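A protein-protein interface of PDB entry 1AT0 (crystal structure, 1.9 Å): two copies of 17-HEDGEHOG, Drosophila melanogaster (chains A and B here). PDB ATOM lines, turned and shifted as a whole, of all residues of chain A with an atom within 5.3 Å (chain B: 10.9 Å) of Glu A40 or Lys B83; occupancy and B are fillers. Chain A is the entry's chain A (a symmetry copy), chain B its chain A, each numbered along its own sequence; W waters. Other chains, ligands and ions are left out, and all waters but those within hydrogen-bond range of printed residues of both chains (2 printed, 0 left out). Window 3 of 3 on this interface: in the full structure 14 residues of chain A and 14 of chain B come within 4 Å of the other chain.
Water W2 lies within hydrogen-bond range of NH1 of Arg A130 and O of Ala B32.
Water W1 lies within hydrogen-bond range of NH1 of Arg A130 (3.4 Å) and O of Thr B85 (3.4 Å).
No position is printed for both chains.
Of the 7 pairs that touch across the chains among the printed residues, none has its exchanged pair printed and touching as well.
The backbone carbonyl oxygen (O) of Thr B85 sits at hydrogen-bond distance from the backbone NH (N) of Val B76, at 2.7 Å.
The side-chain hydroxyl (OG) of Ser A39 sits at hydrogen-bond distance from the backbone NH (N) of Arg A130 (3.1 Å).
The backbone carbonyl oxygen (O) of Lys B83 is in hydrogen-bond range of the backbone NH (N) of Gln B78, 2.8 Å away.
The backbone NH (N) of Ile A42 sits at hydrogen-bond distance from the backbone carbonyl oxygen (O) of Leu A128, 2.8 Å away.
The side-chain carboxylate of Glu A40 is in salt-bridge range of the guanidinium group of Arg A130.
Printed residues of chain B that touch a printed residue of chain A: Leu B73, Lys B83, Leu B84, Thr B85 and Phe B86.
Of the 12 printed residues of chain A, 4 touch a printed residue of chain B.
Printed residues of chain A that touch a printed residue of chain B: Glu A40, Ile A42, Leu A128 and Arg A130.
Among the printed residues, Asp or Glu carboxylates within 4 Å of a Lys or Arg side-chain nitrogen of the other chain: Glu A40 with Lys B83 (3.7 Å).
Among the printed residues, merely in contact across the chains: Arg A130 with Lys B83 (3.6 Å), Arg A130 with Phe B86 (3.8 Å), Arg A130 with Thr B85 (3.9 Å), Leu A128 with Leu B73 (3.9 Å) and Ile A42 with Phe B86 (3.99 Å).
The guanidinium group (NH2) of Arg A130 is in hydrogen-bond range of the backbone carbonyl oxygen (O) of Leu B84, at 2.6 Å.
The side-chain carboxylate (OE2) of Glu A40 lies within salt-bridge range of the side-chain amino group (NZ) of Lys B83.
No residue of chain B comes within 4 Å of Gly A24.
No residue of chain B comes within 4 Å of Arg A26.
No residue of chain B comes within 4 Å of Val A27.
No residue of chain B comes within 4 Å of Val A41.
No residue of chain B comes within 4 Å of Thr A129.
Arg A130 touches four residues of chain B.
Met B30 touches none of the printed residues of chain A.
Printed residues of chain A within 4 Å of Leu B73: Leu A128 (3.9 Å).
Lys B83 touches two residues of chain A.
Printed residues of chain A within 4 Å of Leu B84: Arg A130 (2.6 Å).
Of the printed residues of chain A, Thr B85 touches Arg A130 (3.9 Å).
Printed residues of chain A within 4 Å of Phe B86: Ile A42 (3.99 Å) and Arg A130 (3.8 Å).
The nearest residue of chain B that does not touch Glu A40 is Leu B84 (5.3 Å).
The nearest printed residue of chain A that does not touch Lys B83 is Ile A42 (7.7 Å).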
ATOM      1  N   GLY A  24      13.799  -7.767 -34.021  1.00  0.00           N
ATOM      2  CA  GLY A  24      14.005  -6.964 -32.831  1.00  0.00           C
ATOM      3  C   GLY A  24      13.307  -5.618 -32.948  1.00  0.00           C
ATOM      4  O   GLY A  24      12.870  -5.060 -31.943  1.00  0.00           O
ATOM      5  N   ASP A  25      13.195  -5.095 -34.166  1.00  0.00           N
ATOM      6  CA  ASP A  25      12.522  -3.815 -34.388  1.00  0.00           C
ATOM      7  C   ASP A  25      11.081  -3.924 -33.893  1.00  0.00           C
ATOM      8  O   ASP A  25      10.431  -4.949 -34.096  1.00  0.00           O
ATOM      9  CB  ASP A  25      12.514  -3.452 -35.884  1.00  0.00           C
ATOM     10  CG  ASP A  25      13.895  -3.119 -36.428  1.00  0.00           C
ATOM     11  OD1 ASP A  25      14.872  -3.036 -35.649  1.00  0.00           O
ATOM     12  OD2 ASP A  25      14.015  -2.938 -37.657  1.00  0.00           O
ATOM     13  N   ARG A  26      10.597  -2.895 -33.205  1.00  0.00           N
ATOM     14  CA  ARG A  26       9.225  -2.891 -32.702  1.00  0.00           C
ATOM     15  C   ARG A  26       8.402  -2.064 -33.679  1.00  0.00           C
ATOM     16  O   ARG A  26       8.529  -0.836 -33.747  1.00  0.00           O
ATOM     17  CB  ARG A  26       9.147  -2.299 -31.294  1.00  0.00           C
ATOM     18  CG  ARG A  26      10.045  -2.993 -30.278  1.00  0.00           C
ATOM     19  CD  ARG A  26       9.645  -2.637 -28.852  1.00  0.00           C
ATOM     20  NE  ARG A  26       8.485  -3.406 -28.396  1.00  0.00           N
ATOM     21  CZ  ARG A  26       7.375  -2.870 -27.894  1.00  0.00           C
ATOM     22  NH1 ARG A  26       7.268  -1.555 -27.776  1.00  0.00           N
ATOM     23  NH2 ARG A  26       6.367  -3.653 -27.529  1.00  0.00           N
ATOM     24  N   VAL A  27       7.595  -2.759 -34.467  1.00  0.00           N
ATOM     25  CA  VAL A  27       6.767  -2.131 -35.489  1.00  0.00           C
ATOM     26  C   VAL A  27       5.303  -2.016 -35.083  1.00  0.00           C
ATOM     27  O   VAL A  27       4.825  -2.753 -34.214  1.00  0.00           O
ATOM     28  CB  VAL A  27       6.850  -2.926 -36.811  1.00  0.00           C
ATOM     29  CG1 VAL A  27       8.269  -2.939 -37.322  1.00  0.00           C
ATOM     30  CG2 VAL A  27       6.372  -4.352 -36.596  1.00  0.00           C
ATOM     31  N   TYR A  38       2.583  -1.593 -30.492  1.00  0.00           N
ATOM     32  CA  TYR A  38       3.892  -1.877 -31.070  1.00  0.00           C
ATOM     33  C   TYR A  38       4.348  -3.259 -30.629  1.00  0.00           C
ATOM     34  O   TYR A  38       4.177  -3.630 -29.466  1.00  0.00           O
ATOM     35  CB  TYR A  38       4.896  -0.787 -30.704  1.00  0.00           C
ATOM     36  CG  TYR A  38       4.601   0.497 -31.433  1.00  0.00           C
ATOM     37  CD1 TYR A  38       4.962   0.649 -32.766  1.00  0.00           C
ATOM     38  CD2 TYR A  38       3.894   1.528 -30.818  1.00  0.00           C
ATOM     39  CE1 TYR A  38       4.624   1.790 -33.478  1.00  0.00           C
ATOM     40  CE2 TYR A  38       3.548   2.681 -31.524  1.00  0.00           C
ATOM     41  CZ  TYR A  38       3.918   2.801 -32.855  1.00  0.00           C
ATOM     42  OH  TYR A  38       3.586   3.924 -33.575  1.00  0.00           O
ATOM     43  N   SER A  39       4.885  -4.030 -31.570  1.00  0.00           N
ATOM     44  CA  SER A  39       5.327  -5.393 -31.303  1.00  0.00           C
ATOM     45  C   SER A  39       6.644  -5.647 -32.028  1.00  0.00           C
ATOM     46  O   SER A  39       6.869  -5.110 -33.111  1.00  0.00           O
ATOM     47  CB  SER A  39       4.256  -6.375 -31.806  1.00  0.00           C
ATOM     48  OG  SER A  39       4.519  -7.709 -31.403  1.00  0.00           O
ATOM     49  N   GLU A  40       7.517  -6.461 -31.441  1.00  0.00           N
ATOM     50  CA  GLU A  40       8.795  -6.733 -32.076  1.00  0.00           C
ATOM     51  C   GLU A  40       8.723  -7.814 -33.134  1.00  0.00           C
ATOM     52  O   GLU A  40       7.896  -8.731 -33.062  1.00  0.00           O
ATOM     53  CB  GLU A  40       9.895  -7.061 -31.044  1.00  0.00           C
ATOM     54  CG  GLU A  40       9.812  -8.425 -30.358  1.00  0.00           C
ATOM     55  CD  GLU A  40      10.945  -8.661 -29.351  1.00  0.00           C
ATOM     56  OE1 GLU A  40      11.816  -7.781 -29.197  1.00  0.00           O
ATOM     57  OE2 GLU A  40      10.960  -9.725 -28.686  1.00  0.00           O
ATOM     58  N   VAL A  41       9.543  -7.638 -34.161  1.00  0.00           N
ATOM     59  CA  VAL A  41       9.655  -8.589 -35.251  1.00  0.00           C
ATOM     60  C   VAL A  41      10.506  -9.707 -34.668  1.00  0.00           C
ATOM     61  O   VAL A  41      11.589  -9.449 -34.136  1.00  0.00           O
ATOM     62  CB  VAL A  41      10.402  -7.973 -36.452  1.00  0.00           C
ATOM     63  CG1 VAL A  41      10.660  -9.030 -37.516  1.00  0.00           C
ATOM     64  CG2 VAL A  41       9.601  -6.803 -37.033  1.00  0.00           C
ATOM     65  N   ILE A  42       9.990 -10.929 -34.697  1.00  0.00           N
ATOM     66  CA  ILE A  42      10.723 -12.069 -34.167  1.00  0.00           C
ATOM     67  C   ILE A  42      11.460 -12.834 -35.262  1.00  0.00           C
ATOM     68  O   ILE A  42      12.497 -13.441 -35.008  1.00  0.00           O
ATOM     69  CB  ILE A  42       9.803 -13.006 -33.346  1.00  0.00           C
ATOM     70  CG1 ILE A  42       8.606 -13.461 -34.181  1.00  0.00           C
ATOM     71  CG2 ILE A  42       9.334 -12.292 -32.077  1.00  0.00           C
ATOM     72  CD1 ILE A  42       7.606 -14.296 -33.410  1.00  0.00           C
ATOM     73  N   LEU A 128       7.184 -11.503 -39.170  1.00  0.00           N
ATOM     74  CA  LEU A 128       6.299 -12.036 -38.144  1.00  0.00           C
ATOM     75  C   LEU A 128       6.600 -11.323 -36.832  1.00  0.00           C
ATOM     76  O   LEU A 128       7.737 -11.348 -36.354  1.00  0.00           O
ATOM     77  CB  LEU A 128       6.517 -13.542 -37.973  1.00  0.00           C
ATOM     78  CG  LEU A 128       5.694 -14.222 -36.879  1.00  0.00           C
ATOM     79  CD1 LEU A 128       4.214 -14.144 -37.217  1.00  0.00           C
ATOM     80  CD2 LEU A 128       6.135 -15.673 -36.718  1.00  0.00           C
ATOM     81  N   THR A 129       5.587 -10.681 -36.260  1.00  0.00           N
ATOM     82  CA  THR A 129       5.736  -9.960 -34.994  1.00  0.00           C
ATOM     83  C   THR A 129       5.188 -10.822 -33.848  1.00  0.00           C
ATOM     84  O   THR A 129       4.529 -11.837 -34.100  1.00  0.00           O
ATOM     85  CB  THR A 129       4.936  -8.644 -35.033  1.00  0.00           C
ATOM     86  OG1 THR A 129       3.541  -8.941 -35.191  1.00  0.00           O
ATOM     87  CG2 THR A 129       5.394  -7.769 -36.193  1.00  0.00           C
ATOM     88  N   ARG A 130       5.436 -10.425 -32.599  1.00  0.00           N
ATOM     89  CA  ARG A 130       4.910 -11.179 -31.457  1.00  0.00           C
ATOM     90  C   ARG A 130       3.390 -11.170 -31.454  1.00  0.00           C
ATOM     91  O   ARG A 130       2.759 -12.149 -31.062  1.00  0.00           O
ATOM     92  CB  ARG A 130       5.391 -10.604 -30.130  1.00  0.00           C
ATOM     93  CG  ARG A 130       6.803 -10.964 -29.778  1.00  0.00           C
ATOM     94  CD  ARG A 130       7.130 -10.544 -28.354  1.00  0.00           C
ATOM     95  NE  ARG A 130       8.519 -10.856 -28.071  1.00  0.00           N
ATOM     96  CZ  ARG A 130       8.935 -11.978 -27.495  1.00  0.00           C
ATOM     97  NH1 ARG A 130       8.060 -12.903 -27.109  1.00  0.00           N
ATOM     98  NH2 ARG A 130      10.239 -12.227 -27.423  1.00  0.00           N
ATOM     99  N   MET B  30      -2.377 -17.460 -25.878  1.00  0.00           N
ATOM    100  CA  MET B  30      -1.456 -16.684 -25.051  1.00  0.00           C
ATOM    101  C   MET B  30      -1.238 -15.289 -25.630  1.00  0.00           C
ATOM    102  O   MET B  30      -1.066 -15.128 -26.836  1.00  0.00           O
ATOM    103  CB  MET B  30      -0.113 -17.414 -24.963  1.00  0.00           C
ATOM    104  CG  MET B  30       0.905 -16.737 -24.070  1.00  0.00           C
ATOM    105  SD  MET B  30       2.660 -17.533 -24.269  1.00  0.00           S
ATOM    106  CE  MET B  30       3.115 -16.782 -25.972  1.00  0.00           C
ATOM    107  N   THR B  31      -1.257 -14.281 -24.770  1.00  0.00           N
ATOM    108  CA  THR B  31      -1.042 -12.913 -25.212  1.00  0.00           C
ATOM    109  C   THR B  31       0.454 -12.704 -25.445  1.00  0.00           C
ATOM    110  O   THR B  31       1.269 -13.554 -25.078  1.00  0.00           O
ATOM    111  CB  THR B  31      -1.541 -11.900 -24.163  1.00  0.00           C
ATOM    112  OG1 THR B  31      -0.829 -12.092 -22.936  1.00  0.00           O
ATOM    113  CG2 THR B  31      -3.021 -12.090 -23.909  1.00  0.00           C
ATOM    114  N   ALA B  32       0.815 -11.558 -26.014  1.00  0.00           N
ATOM    115  CA  ALA B  32       2.213 -11.246 -26.288  1.00  0.00           C
ATOM    116  C   ALA B  32       3.049 -11.271 -25.014  1.00  0.00           C
ATOM    117  O   ALA B  32       4.234 -11.598 -25.057  1.00  0.00           O
ATOM    118  CB  ALA B  32       2.334  -9.897 -26.973  1.00  0.00           C
ATOM    119  N   ASN B  33       2.449 -10.927 -23.879  1.00  0.00           N
ATOM    120  CA  ASN B  33       3.194 -10.953 -22.624  1.00  0.00           C
ATOM    121  C   ASN B  33       3.003 -12.246 -21.823  1.00  0.00           C
ATOM    122  O   ASN B  33       3.168 -12.260 -20.602  1.00  0.00           O
ATOM    123  CB  ASN B  33       2.918  -9.706 -21.773  1.00  0.00           C
ATOM    124  CG  ASN B  33       1.480  -9.601 -21.319  1.00  0.00           C
ATOM    125  OD1 ASN B  33       0.595 -10.281 -21.837  1.00  0.00           O
ATOM    126  ND2 ASN B  33       1.235  -8.732 -20.349  1.00  0.00           N
ATOM    127  N   GLY B  34       2.643 -13.321 -22.522  1.00  0.00           N
ATOM    128  CA  GLY B  34       2.478 -14.623 -21.897  1.00  0.00           C
ATOM    129  C   GLY B  34       1.278 -14.926 -21.018  1.00  0.00           C
ATOM    130  O   GLY B  34       1.334 -15.866 -20.224  1.00  0.00           O
ATOM    131  N   LEU B  73       6.976 -23.014 -34.089  1.00  0.00           N
ATOM    132  CA  LEU B  73       7.473 -22.118 -33.039  1.00  0.00           C
ATOM    133  C   LEU B  73       6.794 -22.406 -31.710  1.00  0.00           C
ATOM    134  O   LEU B  73       5.568 -22.541 -31.639  1.00  0.00           O
ATOM    135  CB  LEU B  73       7.246 -20.650 -33.387  1.00  0.00           C
ATOM    136  CG  LEU B  73       8.222 -19.960 -34.327  1.00  0.00           C
ATOM    137  CD1 LEU B  73       7.715 -18.554 -34.564  1.00  0.00           C
ATOM    138  CD2 LEU B  73       9.624 -19.944 -33.725  1.00  0.00           C
ATOM    139  N   VAL B  74       7.594 -22.441 -30.652  1.00  0.00           N
ATOM    140  CA  VAL B  74       7.100 -22.718 -29.314  1.00  0.00           C
ATOM    141  C   VAL B  74       7.666 -21.685 -28.339  1.00  0.00           C
ATOM    142  O   VAL B  74       8.799 -21.230 -28.509  1.00  0.00           O
ATOM    143  CB  VAL B  74       7.501 -24.162 -28.896  1.00  0.00           C
ATOM    144  CG1 VAL B  74       7.191 -24.413 -27.425  1.00  0.00           C
ATOM    145  CG2 VAL B  74       6.774 -25.181 -29.794  1.00  0.00           C
ATOM    146  N   SER B  75       6.852 -21.267 -27.370  1.00  0.00           N
ATOM    147  CA  SER B  75       7.275 -20.291 -26.369  1.00  0.00           C
ATOM    148  C   SER B  75       8.259 -20.918 -25.391  1.00  0.00           C
ATOM    149  O   SER B  75       8.018 -22.012 -24.867  1.00  0.00           O
ATOM    150  CB  SER B  75       6.076 -19.768 -25.579  1.00  0.00           C
ATOM    151  OG  SER B  75       5.134 -19.170 -26.438  1.00  0.00           O
ATOM    152  N   VAL B  76       9.357 -20.214 -25.146  1.00  0.00           N
ATOM    153  CA  VAL B  76      10.394 -20.654 -24.227  1.00  0.00           C
ATOM    154  C   VAL B  76      10.623 -19.513 -23.245  1.00  0.00           C
ATOM    155  O   VAL B  76      10.755 -18.351 -23.636  1.00  0.00           O
ATOM    156  CB  VAL B  76      11.709 -21.000 -24.970  1.00  0.00           C
ATOM    157  CG1 VAL B  76      12.843 -21.213 -23.976  1.00  0.00           C
ATOM    158  CG2 VAL B  76      11.522 -22.258 -25.794  1.00  0.00           C
ATOM    159  N   TRP B  77      10.586 -19.841 -21.964  1.00  0.00           N
ATOM    160  CA  TRP B  77      10.781 -18.856 -20.926  1.00  0.00           C
ATOM    161  C   TRP B  77      12.220 -18.913 -20.437  1.00  0.00           C
ATOM    162  O   TRP B  77      12.751 -19.989 -20.163  1.00  0.00           O
ATOM    163  CB  TRP B  77       9.817 -19.127 -19.771  1.00  0.00           C
ATOM    164  CG  TRP B  77       9.975 -18.194 -18.611  1.00  0.00           C
ATOM    165  CD1 TRP B  77      10.418 -18.512 -17.359  1.00  0.00           C
ATOM    166  CD2 TRP B  77       9.672 -16.794 -18.588  1.00  0.00           C
ATOM    167  NE1 TRP B  77      10.408 -17.398 -16.556  1.00  0.00           N
ATOM    168  CE2 TRP B  77       9.955 -16.329 -17.283  1.00  0.00           C
ATOM    169  CE3 TRP B  77       9.189 -15.887 -19.543  1.00  0.00           C
ATOM    170  CZ2 TRP B  77       9.770 -14.995 -16.906  1.00  0.00           C
ATOM    171  CZ3 TRP B  77       9.004 -14.559 -19.167  1.00  0.00           C
ATOM    172  CH2 TRP B  77       9.294 -14.127 -17.858  1.00  0.00           C
ATOM    173  N   GLN B  78      12.849 -17.748 -20.357  1.00  0.00           N
ATOM    174  CA  GLN B  78      14.223 -17.625 -19.887  1.00  0.00           C
ATOM    175  C   GLN B  78      14.045 -17.063 -18.479  1.00  0.00           C
ATOM    176  O   GLN B  78      13.822 -15.860 -18.298  1.00  0.00           O
ATOM    177  CB  GLN B  78      14.990 -16.640 -20.769  1.00  0.00           C
ATOM    178  CG  GLN B  78      14.572 -16.673 -22.235  1.00  0.00           C
ATOM    179  CD  GLN B  78      15.663 -17.177 -23.149  1.00  0.00           C
ATOM    180  OE1 GLN B  78      15.835 -18.387 -23.327  1.00  0.00           O
ATOM    181  NE2 GLN B  78      16.404 -16.251 -23.747  1.00  0.00           N
ATOM    182  N   PRO B  79      14.111 -17.935 -17.462  1.00  0.00           N
ATOM    183  CA  PRO B  79      13.944 -17.552 -16.057  1.00  0.00           C
ATOM    184  C   PRO B  79      14.844 -16.432 -15.545  1.00  0.00           C
ATOM    185  O   PRO B  79      14.387 -15.572 -14.795  1.00  0.00           O
ATOM    186  CB  PRO B  79      14.178 -18.868 -15.316  1.00  0.00           C
ATOM    187  CG  PRO B  79      15.140 -19.589 -16.213  1.00  0.00           C
ATOM    188  CD  PRO B  79      14.549 -19.338 -17.568  1.00  0.00           C
ATOM    189  N   GLU B  80      16.102 -16.427 -15.967  1.00  0.00           N
ATOM    190  CA  GLU B  80      17.052 -15.418 -15.520  1.00  0.00           C
ATOM    191  C   GLU B  80      16.765 -14.013 -16.025  1.00  0.00           C
ATOM    192  O   GLU B  80      16.784 -13.057 -15.252  1.00  0.00           O
ATOM    193  CB  GLU B  80      18.470 -15.810 -15.920  1.00  0.00           C
ATOM    194  CG  GLU B  80      18.833 -15.507 -17.379  1.00  0.00           C
ATOM    195  CD  GLU B  80      18.021 -16.296 -18.397  1.00  0.00           C
ATOM    196  OE1 GLU B  80      17.553 -17.413 -18.092  1.00  0.00           O
ATOM    197  OE2 GLU B  80      17.850 -15.785 -19.521  1.00  0.00           O
ATOM    198  N   SER B  81      16.505 -13.887 -17.320  1.00  0.00           N
ATOM    199  CA  SER B  81      16.254 -12.588 -17.915  1.00  0.00           C
ATOM    200  C   SER B  81      14.786 -12.232 -18.000  1.00  0.00           C
ATOM    201  O   SER B  81      14.442 -11.193 -18.557  1.00  0.00           O
ATOM    202  CB  SER B  81      16.872 -12.519 -19.313  1.00  0.00           C
ATOM    203  OG  SER B  81      16.304 -13.485 -20.177  1.00  0.00           O
ATOM    204  N   GLN B  82      13.919 -13.085 -17.459  1.00  0.00           N
ATOM    205  CA  GLN B  82      12.484 -12.828 -17.514  1.00  0.00           C
ATOM    206  C   GLN B  82      12.081 -12.547 -18.960  1.00  0.00           C
ATOM    207  O   GLN B  82      11.321 -11.618 -19.242  1.00  0.00           O
ATOM    208  CB  GLN B  82      12.105 -11.625 -16.639  1.00  0.00           C
ATOM    209  CG  GLN B  82      11.675 -11.963 -15.224  1.00  0.00           C
ATOM    210  CD  GLN B  82      12.778 -12.607 -14.432  1.00  0.00           C
ATOM    211  OE1 GLN B  82      13.817 -11.998 -14.190  1.00  0.00           O
ATOM    212  NE2 GLN B  82      12.563 -13.847 -14.022  1.00  0.00           N
ATOM    213  N   LYS B  83      12.616 -13.336 -19.882  1.00  0.00           N
ATOM    214  CA  LYS B  83      12.306 -13.148 -21.286  1.00  0.00           C
ATOM    215  C   LYS B  83      11.512 -14.296 -21.884  1.00  0.00           C
ATOM    216  O   LYS B  83      11.831 -15.467 -21.675  1.00  0.00           O
ATOM    217  CB  LYS B  83      13.587 -12.930 -22.101  1.00  0.00           C
ATOM    218  CG  LYS B  83      14.061 -11.481 -22.160  1.00  0.00           C
ATOM    219  CD  LYS B  83      13.077 -10.584 -22.925  1.00  0.00           C
ATOM    220  CE  LYS B  83      12.954 -10.982 -24.403  1.00  0.00           C
ATOM    221  NZ  LYS B  83      12.038 -10.075 -25.172  1.00  0.00           N
ATOM    222  N   LEU B  84      10.441 -13.945 -22.585  1.00  0.00           N
ATOM    223  CA  LEU B  84       9.613 -14.931 -23.258  1.00  0.00           C
ATOM    224  C   LEU B  84      10.045 -14.859 -24.720  1.00  0.00           C
ATOM    225  O   LEU B  84      10.045 -13.776 -25.323  1.00  0.00           O
ATOM    226  CB  LEU B  84       8.132 -14.573 -23.117  1.00  0.00           C
ATOM    227  CG  LEU B  84       7.124 -15.570 -23.695  1.00  0.00           C
ATOM    228  CD1 LEU B  84       7.252 -16.898 -22.972  1.00  0.00           C
ATOM    229  CD2 LEU B  84       5.703 -15.019 -23.579  1.00  0.00           C
ATOM    230  N   THR B  85      10.499 -15.978 -25.266  1.00  0.00           N
ATOM    231  CA  THR B  85      10.942 -16.010 -26.651  1.00  0.00           C
ATOM    232  C   THR B  85      10.339 -17.200 -27.370  1.00  0.00           C
ATOM    233  O   THR B  85       9.781 -18.095 -26.744  1.00  0.00           O
ATOM    234  CB  THR B  85      12.476 -16.120 -26.744  1.00  0.00           C
ATOM    235  OG1 THR B  85      12.912 -17.287 -26.040  1.00  0.00           O
ATOM    236  CG2 THR B  85      13.142 -14.888 -26.136  1.00  0.00           C
ATOM    237  N   PHE B  86      10.416 -17.186 -28.694  1.00  0.00           N
ATOM    238  CA  PHE B  86       9.900 -18.283 -29.492  1.00  0.00           C
ATOM    239  C   PHE B  86      11.091 -18.993 -30.085  1.00  0.00           C
ATOM    240  O   PHE B  86      12.025 -18.353 -30.563  1.00  0.00           O
ATOM    241  CB  PHE B  86       8.992 -17.770 -30.604  1.00  0.00           C
ATOM    242  CG  PHE B  86       7.671 -17.272 -30.117  1.00  0.00           C
ATOM    243  CD1 PHE B  86       6.589 -18.139 -30.010  1.00  0.00           C
ATOM    244  CD2 PHE B  86       7.501 -15.933 -29.777  1.00  0.00           C
ATOM    245  CE1 PHE B  86       5.356 -17.682 -29.572  1.00  0.00           C
ATOM    246  CE2 PHE B  86       6.273 -15.467 -29.340  1.00  0.00           C
ATOM    247  CZ  PHE B  86       5.196 -16.344 -29.237  1.00  0.00           C
ATOM    248  N   VAL B  87      11.055 -20.318 -30.046  1.00  0.00           N
ATOM    249  CA  VAL B  87      12.135 -21.149 -30.563  1.00  0.00           C
ATOM    250  C   VAL B  87      11.484 -22.278 -31.346  1.00  0.00           C
ATOM    251  O   VAL B  87      10.353 -22.668 -31.044  1.00  0.00           O
ATOM    252  CB  VAL B  87      12.955 -21.757 -29.390  1.00  0.00           C
ATOM    253  CG1 VAL B  87      13.988 -22.748 -29.903  1.00  0.00           C
ATOM    254  CG2 VAL B  87      13.639 -20.652 -28.591  1.00  0.00           C
ATOM    255  N   ASN B  96      15.383 -26.358 -20.794  1.00  0.00           N
ATOM    256  CA  ASN B  96      14.744 -25.133 -21.285  1.00  0.00           C
ATOM    257  C   ASN B  96      13.385 -25.110 -20.588  1.00  0.00           C
ATOM    258  O   ASN B  96      12.939 -26.138 -20.075  1.00  0.00           O
ATOM    259  CB  ASN B  96      14.490 -25.189 -22.798  1.00  0.00           C
ATOM    260  CG  ASN B  96      15.682 -24.744 -23.627  1.00  0.00           C
ATOM    261  OD1 ASN B  96      15.811 -25.136 -24.789  1.00  0.00           O
ATOM    262  ND2 ASN B  96      16.529 -23.895 -23.062  1.00  0.00           N
ATOM    263  N   GLN B  97      12.720 -23.962 -20.569  1.00  0.00           N
ATOM    264  CA  GLN B  97      11.414 -23.875 -19.930  1.00  0.00           C
ATOM    265  C   GLN B  97      10.315 -23.425 -20.891  1.00  0.00           C
ATOM    266  O   GLN B  97      10.542 -22.595 -21.770  1.00  0.00           O
ATOM    267  CB  GLN B  97      11.478 -22.971 -18.697  1.00  0.00           C
ATOM    268  CG  GLN B  97      12.199 -23.633 -17.523  1.00  0.00           C
ATOM    269  CD  GLN B  97      12.314 -22.744 -16.299  1.00  0.00           C
ATOM    270  OE1 GLN B  97      11.320 -22.248 -15.775  1.00  0.00           O
ATOM    271  NE2 GLN B  97      13.530 -22.556 -15.825  1.00  0.00           N
ATOM    272  N   VAL B  98       9.147 -24.048 -20.770  1.00  0.00           N
ATOM    273  CA  VAL B  98       7.997 -23.721 -21.606  1.00  0.00           C
ATOM    274  C   VAL B  98       6.834 -23.351 -20.680  1.00  0.00           C
ATOM    275  O   VAL B  98       6.873 -23.636 -19.481  1.00  0.00           O
ATOM    276  CB  VAL B  98       7.589 -24.911 -22.513  1.00  0.00           C
ATOM    277  CG1 VAL B  98       8.671 -25.182 -23.555  1.00  0.00           C
ATOM    278  CG2 VAL B  98       7.318 -26.153 -21.677  1.00  0.00           C
ATOM    279  N   LEU B  99       5.826 -22.679 -21.221  1.00  0.00           N
ATOM    280  CA  LEU B  99       4.678 -22.275 -20.422  1.00  0.00           C
ATOM    281  C   LEU B  99       3.611 -23.360 -20.455  1.00  0.00           C
ATOM    282  O   LEU B  99       3.207 -23.815 -21.528  1.00  0.00           O
ATOM    283  CB  LEU B  99       4.099 -20.946 -20.919  1.00  0.00           C
ATOM    284  CG  LEU B  99       4.941 -19.677 -20.736  1.00  0.00           C
ATOM    285  CD1 LEU B  99       5.410 -19.565 -19.295  1.00  0.00           C
ATOM    286  CD2 LEU B  99       6.130 -19.707 -21.670  1.00  0.00           C
ATOM    287  N   PRO B 110       5.758 -21.292 -16.195  1.00  0.00           N
ATOM    288  CA  PRO B 110       6.891 -22.056 -16.720  1.00  0.00           C
ATOM    289  C   PRO B 110       7.168 -23.390 -16.035  1.00  0.00           C
ATOM    290  O   PRO B 110       6.997 -23.539 -14.820  1.00  0.00           O
ATOM    291  CB  PRO B 110       8.060 -21.078 -16.586  1.00  0.00           C
ATOM    292  CG  PRO B 110       7.663 -20.220 -15.426  1.00  0.00           C
ATOM    293  CD  PRO B 110       6.199 -19.988 -15.668  1.00  0.00           C
HETATM  294  O   HOH W   1       7.050 -16.086 -26.592  1.00  0.00           O
HETATM  295  O   HOH W   2       5.479 -13.521 -26.917  1.00  0.00           O
